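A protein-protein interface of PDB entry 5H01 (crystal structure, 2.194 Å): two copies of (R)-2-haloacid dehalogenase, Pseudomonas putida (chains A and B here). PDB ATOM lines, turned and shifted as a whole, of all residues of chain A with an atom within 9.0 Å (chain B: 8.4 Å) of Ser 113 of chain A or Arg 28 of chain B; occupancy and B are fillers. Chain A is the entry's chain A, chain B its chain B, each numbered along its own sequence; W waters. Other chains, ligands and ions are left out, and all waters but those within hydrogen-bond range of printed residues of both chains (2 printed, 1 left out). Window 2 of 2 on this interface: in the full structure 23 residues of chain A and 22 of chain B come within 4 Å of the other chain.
Of the 17 printed residues of chain B, 6 touch a printed residue of chain A.
Printed residues of chain B that touch a printed residue of chain A: His 27, Arg 28, Ala 29, Glu 178, His 180 and His 181.
Printed residues of chain A that touch a printed residue of chain B: Met 110, Gly 111, Tyr 112, Ser 113, Arg 115, Glu 116 and Trp 212.
Hydrophobic or aromatic side chains of chain A within 4 Å of the printed part of chain B: Tyr 112 and Trp 212.
Among the printed residues, no Asp or Glu carboxylate lies within 4 Å of a Lys or Arg side-chain nitrogen of the other chain.
No position is printed for both chains.
Of the 14 pairs that touch across the chains among the printed residues, none has its exchanged pair printed and touching as well.
Among the printed residues, merely in contact across the chains: Met 110 of chain A with His 180 of chain B, Tyr 112 of chain A with His 181 of chain B, Tyr 112 of chain A with His 180 of chain B, Trp 212 of chain A with His 181 of chain B, Ser 113 of chain A with Arg 28 of chain B and Glu 116 of chain A with Glu 178 of chain B.
OG of Ser 34 of chain B lies close to O of Ala 29 of chain B (3.4 Å).
A ring nitrogen (NE2) of His 181 of chain B is in hydrogen-bond range of a ring nitrogen (NE2) of His 180 of chain B (3.4 Å).
N of Tyr 112 of chain A lies within hydrogen-bond range of O of Leu 107 of chain A (3.0 Å).
The side-chain carboxylate (OE1) of Glu 116 of chain A lies within hydrogen-bond range of the backbone NH (N) of Ser 113 of chain A, at 3.1 Å.
The backbone carbonyl oxygen of Arg 115 of chain A lies close to the side-chain amide nitrogen of Gln 119 of chain A (3.4 Å).
The backbone NH (N) of Glu 178 of chain B sits at hydrogen-bond distance from a ring nitrogen (ND1) of His 181 of chain B (3.3 Å).
Of chain B, only His 27 and Arg 28 come within 4 Å of Ser 113 of chain A.
Arg 28 of chain B touches two residues of chain A.
His 27 of chain B touches just these residues of chain A: Ser 113, Arg 115 and Glu 116.
Ala 29 of chain B touches just one residue of chain A: Arg 115.
Of the printed residues of chain B, Met 110 of chain A touches His 180.
Printed residues of chain A within 4 Å of His 180 of chain B: Met 110, Gly 111, Tyr 112 and Glu 116.
Of the printed residues of chain B, Arg 115 of chain A touches His 27 (3.2 Å) and Ala 29 (3.1 Å).
Printed residues of chain B within 4 Å of Gly 111 of chain A: Arg 28 (2.7 Å) and His 180 (3.2 Å).
Printed residues of chain B within 4 Å of Tyr 112 of chain A: His 180 (3.7 Å) and His 181 (3.6 Å).
The nearest residue of chain A that does not touch Arg 28 of chain B is Tyr 112 of chain A (4.5 Å).
The nearest printed residue of chain A that does not touch His 180 of chain B is Ser 113 of chain A (4.9 Å).
Water W1 lies within hydrogen-bond range of O of His 27 of chain B (2.6 Å), N of Arg 115 of chain A (3.0 Å) and OG of Ser 113 of chain A (3.3 Å).
Water W2 lies within hydrogen-bond range of O of His 180 of chain B and O of Met 110 of chain A.
NE2 of His 181 of chain B sits at hydrogen-bond distance from OE2 of Glu 116 of chain A (2.7 Å).
NE of Arg 115 of chain A lies within hydrogen-bond range of O of His 27 of chain B (3.2 Å).
The side-chain carboxylate (OE1) of Glu 116 of chain A lies within hydrogen-bond range of a ring nitrogen (NE2) of His 180 of chain B (2.9 Å).
A ring nitrogen (NE2) of His 180 of chain B is in hydrogen-bond range of the backbone carbonyl oxygen (O) of Gly 111 of chain A, 3.2 Å away.
A ring nitrogen (ND1) of His 27 of chain B lies within hydrogen-bond range of the side-chain hydroxyl (OG) of Ser 113 of chain A, 2.7 Å away.
O of Gly 111 of chain A is in hydrogen-bond range of NH2 of Arg 28 of chain B (2.7 Å).
A ring nitrogen (NE2) of His 27 of chain B lies within hydrogen-bond range of the side-chain carboxylate (OE2) of Glu 116 of chain A (3.3 Å).
The backbone carbonyl oxygen of Ala 29 of chain B sits at hydrogen-bond distance from the guanidinium group of Arg 115 of chain A, at 3.1 Å.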
ATOM      1  N   THR A 104      23.509 -14.295 -11.573  1.00  0.00           N
ATOM      2  CA  THR A 104      23.900 -15.689 -11.706  1.00  0.00           C
ATOM      3  C   THR A 104      25.010 -16.071 -10.717  1.00  0.00           C
ATOM      4  O   THR A 104      25.149 -17.238 -10.362  1.00  0.00           O
ATOM      5  CB  THR A 104      24.379 -16.002 -13.143  1.00  0.00           C
ATOM      6  OG1 THR A 104      25.507 -15.179 -13.472  1.00  0.00           O
ATOM      7  CG2 THR A 104      23.270 -15.739 -14.130  1.00  0.00           C
ATOM      8  N   LEU A 107      23.296 -16.960  -7.564  1.00  0.00           N
ATOM      9  CA  LEU A 107      22.588 -18.225  -7.698  1.00  0.00           C
ATOM     10  C   LEU A 107      23.610 -19.339  -7.485  1.00  0.00           C
ATOM     11  O   LEU A 107      23.341 -20.326  -6.792  1.00  0.00           O
ATOM     12  CB  LEU A 107      21.899 -18.331  -9.064  1.00  0.00           C
ATOM     13  CG  LEU A 107      20.529 -17.641  -9.200  1.00  0.00           C
ATOM     14  CD1 LEU A 107      19.832 -18.022 -10.501  1.00  0.00           C
ATOM     15  CD2 LEU A 107      19.625 -17.940  -8.007  1.00  0.00           C
ATOM     16  N   ARG A 108      24.794 -19.144  -8.062  1.00  0.00           N
ATOM     17  CA  ARG A 108      25.901 -20.083  -7.897  1.00  0.00           C
ATOM     18  C   ARG A 108      26.239 -20.262  -6.416  1.00  0.00           C
ATOM     19  O   ARG A 108      26.415 -21.387  -5.935  1.00  0.00           O
ATOM     20  CB  ARG A 108      27.135 -19.607  -8.663  1.00  0.00           C
ATOM     21  CG  ARG A 108      28.406 -20.239  -8.133  1.00  0.00           C
ATOM     22  CD  ARG A 108      29.663 -19.444  -8.466  1.00  0.00           C
ATOM     23  NE  ARG A 108      30.843 -20.143  -7.961  1.00  0.00           N
ATOM     24  CZ  ARG A 108      31.086 -20.389  -6.672  1.00  0.00           C
ATOM     25  NH1 ARG A 108      30.253 -19.964  -5.723  1.00  0.00           N
ATOM     26  NH2 ARG A 108      32.186 -21.044  -6.322  1.00  0.00           N
ATOM     27  N   GLU A 109      26.298 -19.151  -5.688  1.00  0.00           N
ATOM     28  CA  GLU A 109      26.636 -19.197  -4.268  1.00  0.00           C
ATOM     29  C   GLU A 109      25.543 -19.850  -3.447  1.00  0.00           C
ATOM     30  O   GLU A 109      25.820 -20.428  -2.403  1.00  0.00           O
ATOM     31  CB  GLU A 109      26.929 -17.793  -3.735  1.00  0.00           C
ATOM     32  CG  GLU A 109      28.146 -17.148  -4.389  1.00  0.00           C
ATOM     33  CD  GLU A 109      28.480 -15.796  -3.802  1.00  0.00           C
ATOM     34  OE1 GLU A 109      27.875 -15.427  -2.766  1.00  0.00           O
ATOM     35  OE2 GLU A 109      29.363 -15.117  -4.373  1.00  0.00           O
ATOM     36  N   MET A 110      24.303 -19.742  -3.918  1.00  0.00           N
ATOM     37  CA  MET A 110      23.169 -20.411  -3.289  1.00  0.00           C
ATOM     38  C   MET A 110      23.248 -21.913  -3.528  1.00  0.00           C
ATOM     39  O   MET A 110      22.642 -22.696  -2.798  1.00  0.00           O
ATOM     40  CB  MET A 110      21.841 -19.855  -3.823  1.00  0.00           C
ATOM     41  CG  MET A 110      21.583 -18.400  -3.460  1.00  0.00           C
ATOM     42  SD  MET A 110      20.121 -17.678  -4.241  1.00  0.00           S
ATOM     43  CE  MET A 110      18.835 -18.734  -3.580  1.00  0.00           C
ATOM     44  N   GLY A 111      23.990 -22.313  -4.555  1.00  0.00           N
ATOM     45  CA  GLY A 111      24.208 -23.725  -4.801  1.00  0.00           C
ATOM     46  C   GLY A 111      23.739 -24.206  -6.156  1.00  0.00           C
ATOM     47  O   GLY A 111      23.782 -25.403  -6.448  1.00  0.00           O
ATOM     48  N   TYR A 112      23.290 -23.278  -6.992  1.00  0.00           N
ATOM     49  CA  TYR A 112      22.759 -23.643  -8.299  1.00  0.00           C
ATOM     50  C   TYR A 112      23.914 -23.960  -9.236  1.00  0.00           C
ATOM     51  O   TYR A 112      24.899 -23.227  -9.260  1.00  0.00           O
ATOM     52  CB  TYR A 112      21.890 -22.509  -8.873  1.00  0.00           C
ATOM     53  CG  TYR A 112      20.479 -22.449  -8.315  1.00  0.00           C
ATOM     54  CD1 TYR A 112      20.209 -21.841  -7.092  1.00  0.00           C
ATOM     55  CD2 TYR A 112      19.421 -22.998  -9.020  1.00  0.00           C
ATOM     56  CE1 TYR A 112      18.908 -21.778  -6.585  1.00  0.00           C
ATOM     57  CE2 TYR A 112      18.116 -22.951  -8.523  1.00  0.00           C
ATOM     58  CZ  TYR A 112      17.869 -22.335  -7.312  1.00  0.00           C
ATOM     59  OH  TYR A 112      16.585 -22.291  -6.831  1.00  0.00           O
ATOM     60  N   SER A 113      23.805 -25.044 -10.003  1.00  0.00           N
ATOM     61  CA  SER A 113      24.877 -25.400 -10.941  1.00  0.00           C
ATOM     62  C   SER A 113      24.695 -24.707 -12.283  1.00  0.00           C
ATOM     63  O   SER A 113      23.641 -24.112 -12.559  1.00  0.00           O
ATOM     64  CB  SER A 113      24.958 -26.922 -11.144  1.00  0.00           C
ATOM     65  OG  SER A 113      23.846 -27.396 -11.876  1.00  0.00           O
ATOM     66  N   VAL A 114      25.721 -24.790 -13.119  1.00  0.00           N
ATOM     67  CA  VAL A 114      25.683 -24.170 -14.434  1.00  0.00           C
ATOM     68  C   VAL A 114      24.533 -24.724 -15.277  1.00  0.00           C
ATOM     69  O   VAL A 114      23.926 -23.991 -16.067  1.00  0.00           O
ATOM     70  CB  VAL A 114      27.034 -24.360 -15.166  1.00  0.00           C
ATOM     71  CG1 VAL A 114      26.860 -24.281 -16.676  1.00  0.00           C
ATOM     72  CG2 VAL A 114      28.031 -23.319 -14.682  1.00  0.00           C
ATOM     73  N   ARG A 115      24.213 -26.003 -15.077  1.00  0.00           N
ATOM     74  CA  ARG A 115      23.137 -26.664 -15.827  1.00  0.00           C
ATOM     75  C   ARG A 115      21.742 -26.201 -15.382  1.00  0.00           C
ATOM     76  O   ARG A 115      20.868 -25.986 -16.208  1.00  0.00           O
ATOM     77  CB  ARG A 115      23.263 -28.188 -15.696  1.00  0.00           C
ATOM     78  CG  ARG A 115      24.079 -28.829 -16.830  1.00  0.00           C
ATOM     79  CD  ARG A 115      24.163 -30.343 -16.684  1.00  0.00           C
ATOM     80  NE  ARG A 115      25.538 -30.772 -16.426  1.00  0.00           N
ATOM     81  CZ  ARG A 115      26.428 -31.057 -17.373  1.00  0.00           C
ATOM     82  NH1 ARG A 115      26.084 -31.007 -18.653  1.00  0.00           N
ATOM     83  NH2 ARG A 115      27.658 -31.433 -17.039  1.00  0.00           N
ATOM     84  N   GLU A 116      21.550 -26.043 -14.077  1.00  0.00           N
ATOM     85  CA  GLU A 116      20.290 -25.570 -13.535  1.00  0.00           C
ATOM     86  C   GLU A 116      19.990 -24.144 -13.958  1.00  0.00           C
ATOM     87  O   GLU A 116      18.848 -23.812 -14.302  1.00  0.00           O
ATOM     88  CB  GLU A 116      20.317 -25.667 -12.015  1.00  0.00           C
ATOM     89  CG  GLU A 116      20.620 -27.069 -11.485  1.00  0.00           C
ATOM     90  CD  GLU A 116      20.412 -27.163  -9.995  1.00  0.00           C
ATOM     91  OE1 GLU A 116      21.051 -26.364  -9.283  1.00  0.00           O
ATOM     92  OE2 GLU A 116      19.621 -28.025  -9.532  1.00  0.00           O
ATOM     93  N   ILE A 117      21.009 -23.292 -13.918  1.00  0.00           N
ATOM     94  CA  ILE A 117      20.850 -21.914 -14.344  1.00  0.00           C
ATOM     95  C   ILE A 117      20.521 -21.890 -15.841  1.00  0.00           C
ATOM     96  O   ILE A 117      19.756 -21.039 -16.295  1.00  0.00           O
ATOM     97  CB  ILE A 117      22.107 -21.077 -14.042  1.00  0.00           C
ATOM     98  CG1 ILE A 117      22.261 -20.924 -12.530  1.00  0.00           C
ATOM     99  CG2 ILE A 117      21.988 -19.680 -14.651  1.00  0.00           C
ATOM    100  CD1 ILE A 117      23.689 -20.564 -12.079  1.00  0.00           C
ATOM    101  N   GLY A 118      21.064 -22.846 -16.596  1.00  0.00           N
ATOM    102  CA  GLY A 118      20.653 -23.034 -17.980  1.00  0.00           C
ATOM    103  C   GLY A 118      19.162 -23.331 -18.151  1.00  0.00           C
ATOM    104  O   GLY A 118      18.495 -22.696 -18.981  1.00  0.00           O
ATOM    105  N   GLN A 119      18.640 -24.275 -17.365  1.00  0.00           N
ATOM    106  CA  GLN A 119      17.228 -24.702 -17.449  1.00  0.00           C
ATOM    107  C   GLN A 119      16.282 -23.574 -17.078  1.00  0.00           C
ATOM    108  O   GLN A 119      15.174 -23.470 -17.611  1.00  0.00           O
ATOM    109  CB  GLN A 119      16.953 -25.904 -16.521  1.00  0.00           C
ATOM    110  CG  GLN A 119      17.954 -27.029 -16.627  1.00  0.00           C
ATOM    111  CD  GLN A 119      17.891 -27.989 -15.436  1.00  0.00           C
ATOM    112  OE1 GLN A 119      16.870 -28.098 -14.763  1.00  0.00           O
ATOM    113  NE2 GLN A 119      18.992 -28.666 -15.166  1.00  0.00           N
ATOM    114  N   ILE A 120      16.721 -22.773 -16.113  1.00  0.00           N
ATOM    115  CA  ILE A 120      15.990 -21.612 -15.647  1.00  0.00           C
ATOM    116  C   ILE A 120      15.890 -20.555 -16.740  1.00  0.00           C
ATOM    117  O   ILE A 120      14.836 -19.928 -16.928  1.00  0.00           O
ATOM    118  CB  ILE A 120      16.668 -21.005 -14.398  1.00  0.00           C
ATOM    119  CG1 ILE A 120      16.408 -21.859 -13.163  1.00  0.00           C
ATOM    120  CG2 ILE A 120      16.180 -19.585 -14.138  1.00  0.00           C
ATOM    121  CD1 ILE A 120      17.152 -21.342 -11.913  1.00  0.00           C
ATOM    122  N   ARG A 121      16.987 -20.341 -17.455  1.00  0.00           N
ATOM    123  CA  ARG A 121      16.974 -19.385 -18.561  1.00  0.00           C
ATOM    124  C   ARG A 121      16.045 -19.890 -19.650  1.00  0.00           C
ATOM    125  O   ARG A 121      15.332 -19.102 -20.292  1.00  0.00           O
ATOM    126  CB  ARG A 121      18.373 -19.179 -19.137  1.00  0.00           C
ATOM    127  CG  ARG A 121      19.369 -18.520 -18.217  1.00  0.00           C
ATOM    128  CD  ARG A 121      20.581 -18.093 -19.032  1.00  0.00           C
ATOM    129  NE  ARG A 121      21.570 -17.421 -18.206  1.00  0.00           N
ATOM    130  CZ  ARG A 121      22.665 -18.005 -17.732  1.00  0.00           C
ATOM    131  NH1 ARG A 121      22.909 -19.284 -18.007  1.00  0.00           N
ATOM    132  NH2 ARG A 121      23.507 -17.312 -16.978  1.00  0.00           N
ATOM    133  N   TRP A 212      11.494 -23.497  -8.906  1.00  0.00           N
ATOM    134  CA  TRP A 212      12.700 -23.133  -8.176  1.00  0.00           C
ATOM    135  C   TRP A 212      12.405 -22.054  -7.141  1.00  0.00           C
ATOM    136  O   TRP A 212      12.702 -20.881  -7.363  1.00  0.00           O
ATOM    137  CB  TRP A 212      13.771 -22.642  -9.146  1.00  0.00           C
ATOM    138  CG  TRP A 212      14.252 -23.679 -10.127  1.00  0.00           C
ATOM    139  CD1 TRP A 212      15.122 -24.704  -9.877  1.00  0.00           C
ATOM    140  CD2 TRP A 212      13.903 -23.773 -11.523  1.00  0.00           C
ATOM    141  NE1 TRP A 212      15.333 -25.435 -11.034  1.00  0.00           N
ATOM    142  CE2 TRP A 212      14.604 -24.881 -12.052  1.00  0.00           C
ATOM    143  CE3 TRP A 212      13.065 -23.029 -12.369  1.00  0.00           C
ATOM    144  CZ2 TRP A 212      14.483 -25.268 -13.400  1.00  0.00           C
ATOM    145  CZ3 TRP A 212      12.960 -23.414 -13.715  1.00  0.00           C
ATOM    146  CH2 TRP A 212      13.668 -24.526 -14.209  1.00  0.00           C
ATOM    147  N   PRO B  23      27.457 -36.492  -2.267  1.00  0.00           N
ATOM    148  CA  PRO B  23      26.782 -36.859  -3.524  1.00  0.00           C
ATOM    149  C   PRO B  23      27.195 -35.992  -4.702  1.00  0.00           C
ATOM    150  O   PRO B  23      27.359 -34.780  -4.540  1.00  0.00           O
ATOM    151  CB  PRO B  23      25.298 -36.643  -3.214  1.00  0.00           C
ATOM    152  CG  PRO B  23      25.191 -36.709  -1.712  1.00  0.00           C
ATOM    153  CD  PRO B  23      26.498 -36.152  -1.197  1.00  0.00           C
ATOM    154  N   VAL B  24      27.380 -36.612  -5.866  1.00  0.00           N
ATOM    155  CA  VAL B  24      27.493 -35.866  -7.113  1.00  0.00           C
ATOM    156  C   VAL B  24      26.164 -35.968  -7.865  1.00  0.00           C
ATOM    157  O   VAL B  24      25.891 -36.987  -8.518  1.00  0.00           O
ATOM    158  CB  VAL B  24      28.624 -36.395  -8.000  1.00  0.00           C
ATOM    159  CG1 VAL B  24      28.750 -35.543  -9.258  1.00  0.00           C
ATOM    160  CG2 VAL B  24      29.941 -36.408  -7.241  1.00  0.00           C
ATOM    161  N   PRO B  25      25.324 -34.917  -7.786  1.00  0.00           N
ATOM    162  CA  PRO B  25      24.023 -35.072  -8.467  1.00  0.00           C
ATOM    163  C   PRO B  25      24.175 -35.057  -9.987  1.00  0.00           C
ATOM    164  O   PRO B  25      25.285 -34.785 -10.468  1.00  0.00           O
ATOM    165  CB  PRO B  25      23.204 -33.888  -7.958  1.00  0.00           C
ATOM    166  CG  PRO B  25      24.209 -32.849  -7.548  1.00  0.00           C
ATOM    167  CD  PRO B  25      25.479 -33.594  -7.144  1.00  0.00           C
ATOM    168  N   GLU B  26      23.110 -35.375 -10.722  1.00  0.00           N
ATOM    169  CA  GLU B  26      23.217 -35.536 -12.168  1.00  0.00           C
ATOM    170  C   GLU B  26      23.428 -34.204 -12.874  1.00  0.00           C
ATOM    171  O   GLU B  26      23.976 -34.159 -13.979  1.00  0.00           O
ATOM    172  CB  GLU B  26      21.975 -36.222 -12.740  1.00  0.00           C
ATOM    173  CG  GLU B  26      21.848 -37.663 -12.357  1.00  0.00           C
ATOM    174  CD  GLU B  26      20.614 -38.332 -12.915  1.00  0.00           C
ATOM    175  OE1 GLU B  26      20.571 -38.606 -14.137  1.00  0.00           O
ATOM    176  OE2 GLU B  26      19.697 -38.629 -12.114  1.00  0.00           O
ATOM    177  N   HIS B  27      23.010 -33.116 -12.246  1.00  0.00           N
ATOM    178  CA  HIS B  27      23.151 -31.824 -12.904  1.00  0.00           C
ATOM    179  C   HIS B  27      24.542 -31.237 -12.688  1.00  0.00           C
ATOM    180  O   HIS B  27      24.899 -30.243 -13.302  1.00  0.00           O
ATOM    181  CB  HIS B  27      22.067 -30.858 -12.432  1.00  0.00           C
ATOM    182  CG  HIS B  27      22.115 -30.534 -10.972  1.00  0.00           C
ATOM    183  ND1 HIS B  27      22.829 -29.464 -10.470  1.00  0.00           N
ATOM    184  CD2 HIS B  27      21.505 -31.116  -9.909  1.00  0.00           C
ATOM    185  CE1 HIS B  27      22.657 -29.402  -9.160  1.00  0.00           C
ATOM    186  NE2 HIS B  27      21.865 -30.396  -8.795  1.00  0.00           N
ATOM    187  N   ARG B  28      25.332 -31.874 -11.833  1.00  0.00           N
ATOM    188  CA  ARG B  28      26.736 -31.494 -11.666  1.00  0.00           C
ATOM    189  C   ARG B  28      27.712 -32.499 -12.284  1.00  0.00           C
ATOM    190  O   ARG B  28      28.886 -32.184 -12.469  1.00  0.00           O
ATOM    191  CB  ARG B  28      27.080 -31.325 -10.183  1.00  0.00           C
ATOM    192  CG  ARG B  28      26.406 -30.170  -9.468  1.00  0.00           C
ATOM    193  CD  ARG B  28      27.002 -30.016  -8.074  1.00  0.00           C
ATOM    194  NE  ARG B  28      26.394 -28.971  -7.254  1.00  0.00           N
ATOM    195  CZ  ARG B  28      26.678 -27.672  -7.353  1.00  0.00           C
ATOM    196  NH1 ARG B  28      27.533 -27.222  -8.272  1.00  0.00           N
ATOM    197  NH2 ARG B  28      26.083 -26.807  -6.544  1.00  0.00           N
ATOM    198  N   ALA B  29      27.240 -33.706 -12.587  1.00  0.00           N
ATOM    199  CA  ALA B  29      28.140 -34.794 -13.007  1.00  0.00           C
ATOM    200  C   ALA B  29      28.964 -34.412 -14.235  1.00  0.00           C
ATOM    201  O   ALA B  29      28.433 -33.782 -15.149  1.00  0.00           O
ATOM    202  CB  ALA B  29      27.345 -36.066 -13.289  1.00  0.00           C
ATOM    203  N   ASP B  30      30.254 -34.767 -14.261  1.00  0.00           N
ATOM    204  CA  ASP B  30      31.056 -34.464 -15.451  1.00  0.00           C
ATOM    205  C   ASP B  30      30.791 -35.537 -16.494  1.00  0.00           C
ATOM    206  O   ASP B  30      29.958 -36.417 -16.265  1.00  0.00           O
ATOM    207  CB  ASP B  30      32.565 -34.317 -15.138  1.00  0.00           C
ATOM    208  CG  ASP B  30      33.212 -35.586 -14.580  1.00  0.00           C
ATOM    209  OD1 ASP B  30      32.748 -36.711 -14.864  1.00  0.00           O
ATOM    210  OD2 ASP B  30      34.239 -35.451 -13.879  1.00  0.00           O
ATOM    211  N   GLN B  31      31.475 -35.477 -17.632  1.00  0.00           N
ATOM    212  CA  GLN B  31      31.091 -36.321 -18.758  1.00  0.00           C
ATOM    213  C   GLN B  31      31.426 -37.788 -18.509  1.00  0.00           C
ATOM    214  O   GLN B  31      30.687 -38.677 -18.935  1.00  0.00           O
ATOM    215  CB  GLN B  31      31.749 -35.824 -20.045  1.00  0.00           C
ATOM    216  CG  GLN B  31      32.165 -34.358 -19.986  1.00  0.00           C
ATOM    217  CD  GLN B  31      32.352 -33.729 -21.362  1.00  0.00           C
ATOM    218  OE1 GLN B  31      31.713 -34.128 -22.340  1.00  0.00           O
ATOM    219  NE2 GLN B  31      33.244 -32.747 -21.442  1.00  0.00           N
ATOM    220  N   LEU B  33      31.644 -39.360 -15.428  1.00  0.00           N
ATOM    221  CA  LEU B  33      30.661 -39.820 -14.461  1.00  0.00           C
ATOM    222  C   LEU B  33      29.276 -40.018 -15.113  1.00  0.00           C
ATOM    223  O   LEU B  33      28.623 -41.042 -14.902  1.00  0.00           O
ATOM    224  CB  LEU B  33      30.589 -38.819 -13.299  1.00  0.00           C
ATOM    225  CG  LEU B  33      29.933 -39.201 -11.970  1.00  0.00           C
ATOM    226  CD1 LEU B  33      30.287 -40.642 -11.567  1.00  0.00           C
ATOM    227  CD2 LEU B  33      30.373 -38.218 -10.882  1.00  0.00           C
ATOM    228  N   SER B  34      28.845 -39.053 -15.919  1.00  0.00           N
ATOM    229  CA  SER B  34      27.536 -39.120 -16.561  1.00  0.00           C
ATOM    230  C   SER B  34      27.386 -40.339 -17.474  1.00  0.00           C
ATOM    231  O   SER B  34      26.271 -40.833 -17.679  1.00  0.00           O
ATOM    232  CB  SER B  34      27.276 -37.831 -17.351  1.00  0.00           C
ATOM    233  OG  SER B  34      27.299 -36.716 -16.478  1.00  0.00           O
ATOM    234  N   TYR B  37      26.642 -43.034 -15.006  1.00  0.00           N
ATOM    235  CA  TYR B  37      25.276 -42.691 -14.597  1.00  0.00           C
ATOM    236  C   TYR B  37      24.261 -43.133 -15.631  1.00  0.00           C
ATOM    237  O   TYR B  37      23.171 -43.573 -15.289  1.00  0.00           O
ATOM    238  CB  TYR B  37      25.146 -41.189 -14.343  1.00  0.00           C
ATOM    239  CG  TYR B  37      25.606 -40.751 -12.969  1.00  0.00           C
ATOM    240  CD1 TYR B  37      26.235 -41.645 -12.111  1.00  0.00           C
ATOM    241  CD2 TYR B  37      25.399 -39.455 -12.525  1.00  0.00           C
ATOM    242  CE1 TYR B  37      26.655 -41.263 -10.844  1.00  0.00           C
ATOM    243  CE2 TYR B  37      25.815 -39.058 -11.256  1.00  0.00           C
ATOM    244  CZ  TYR B  37      26.446 -39.976 -10.422  1.00  0.00           C
ATOM    245  OH  TYR B  37      26.858 -39.600  -9.162  1.00  0.00           O
ATOM    246  N   GLN B  54      24.944 -41.686  -6.173  1.00  0.00           N
ATOM    247  CA  GLN B  54      25.552 -40.355  -6.217  1.00  0.00           C
ATOM    248  C   GLN B  54      26.675 -40.261  -5.169  1.00  0.00           C
ATOM    249  O   GLN B  54      27.652 -39.533  -5.359  1.00  0.00           O
ATOM    250  CB  GLN B  54      24.525 -39.233  -5.967  1.00  0.00           C
ATOM    251  CG  GLN B  54      23.547 -38.959  -7.103  1.00  0.00           C
ATOM    252  CD  GLN B  54      22.391 -38.044  -6.682  1.00  0.00           C
ATOM    253  OE1 GLN B  54      22.608 -36.949  -6.147  1.00  0.00           O
ATOM    254  NE2 GLN B  54      21.153 -38.508  -6.905  1.00  0.00           N
ATOM    255  N   ARG B  60      34.971 -42.814  -6.866  1.00  0.00           N
ATOM    256  CA  ARG B  60      34.637 -43.195  -8.246  1.00  0.00           C
ATOM    257  C   ARG B  60      35.308 -44.438  -8.853  1.00  0.00           C
ATOM    258  O   ARG B  60      34.647 -45.187  -9.586  1.00  0.00           O
ATOM    259  CB  ARG B  60      34.898 -42.002  -9.177  1.00  0.00           C
ATOM    260  CG  ARG B  60      34.071 -42.061 -10.459  1.00  0.00           C
ATOM    261  CD  ARG B  60      34.465 -40.941 -11.395  1.00  0.00           C
ATOM    262  NE  ARG B  60      34.119 -39.639 -10.838  1.00  0.00           N
ATOM    263  CZ  ARG B  60      34.071 -38.523 -11.552  1.00  0.00           C
ATOM    264  NH1 ARG B  60      34.357 -38.567 -12.846  1.00  0.00           N
ATOM    265  NH2 ARG B  60      33.745 -37.367 -10.978  1.00  0.00           N
ATOM    266  N   GLU B 178      15.463 -29.889  -5.324  1.00  0.00           N
ATOM    267  CA  GLU B 178      16.687 -29.949  -4.511  1.00  0.00           C
ATOM    268  C   GLU B 178      16.629 -29.049  -3.272  1.00  0.00           C
ATOM    269  O   GLU B 178      15.764 -28.177  -3.165  1.00  0.00           O
ATOM    270  CB  GLU B 178      17.909 -29.557  -5.356  1.00  0.00           C
ATOM    271  CG  GLU B 178      18.041 -30.328  -6.673  1.00  0.00           C
ATOM    272  CD  GLU B 178      18.243 -31.828  -6.491  1.00  0.00           C
ATOM    273  OE1 GLU B 178      18.800 -32.243  -5.445  1.00  0.00           O
ATOM    274  OE2 GLU B 178      17.865 -32.594  -7.414  1.00  0.00           O
ATOM    275  N   HIS B 180      18.561 -26.690  -2.246  1.00  0.00           N
ATOM    276  CA  HIS B 180      18.894 -25.276  -2.426  1.00  0.00           C
ATOM    277  C   HIS B 180      17.840 -24.575  -3.288  1.00  0.00           C
ATOM    278  O   HIS B 180      17.856 -23.347  -3.451  1.00  0.00           O
ATOM    279  CB  HIS B 180      20.294 -25.118  -3.034  1.00  0.00           C
ATOM    280  CG  HIS B 180      20.489 -25.853  -4.323  1.00  0.00           C
ATOM    281  ND1 HIS B 180      20.584 -27.221  -4.399  1.00  0.00           N
ATOM    282  CD2 HIS B 180      20.619 -25.402  -5.602  1.00  0.00           C
ATOM    283  CE1 HIS B 180      20.764 -27.589  -5.656  1.00  0.00           C
ATOM    284  NE2 HIS B 180      20.780 -26.500  -6.403  1.00  0.00           N
ATOM    285  N   HIS B 181      16.934 -25.373  -3.846  1.00  0.00           N
ATOM    286  CA  HIS B 181      15.749 -24.878  -4.528  1.00  0.00           C
ATOM    287  C   HIS B 181      14.695 -24.444  -3.511  1.00  0.00           C
ATOM    288  O   HIS B 181      13.901 -23.522  -3.746  1.00  0.00           O
ATOM    289  CB  HIS B 181      15.149 -25.963  -5.430  1.00  0.00           C
ATOM    290  CG  HIS B 181      16.073 -26.475  -6.490  1.00  0.00           C
ATOM    291  ND1 HIS B 181      15.668 -27.389  -7.442  1.00  0.00           N
ATOM    292  CD2 HIS B 181      17.378 -26.220  -6.744  1.00  0.00           C
ATOM    293  CE1 HIS B 181      16.674 -27.653  -8.251  1.00  0.00           C
ATOM    294  NE2 HIS B 181      17.728 -26.970  -7.847  1.00  0.00           N
HETATM  295  O   HOH W   1      26.130 -28.128 -14.158  1.00  0.00           O
HETATM  296  O   HOH W   2      19.755 -21.669  -1.864  1.00  0.00           O
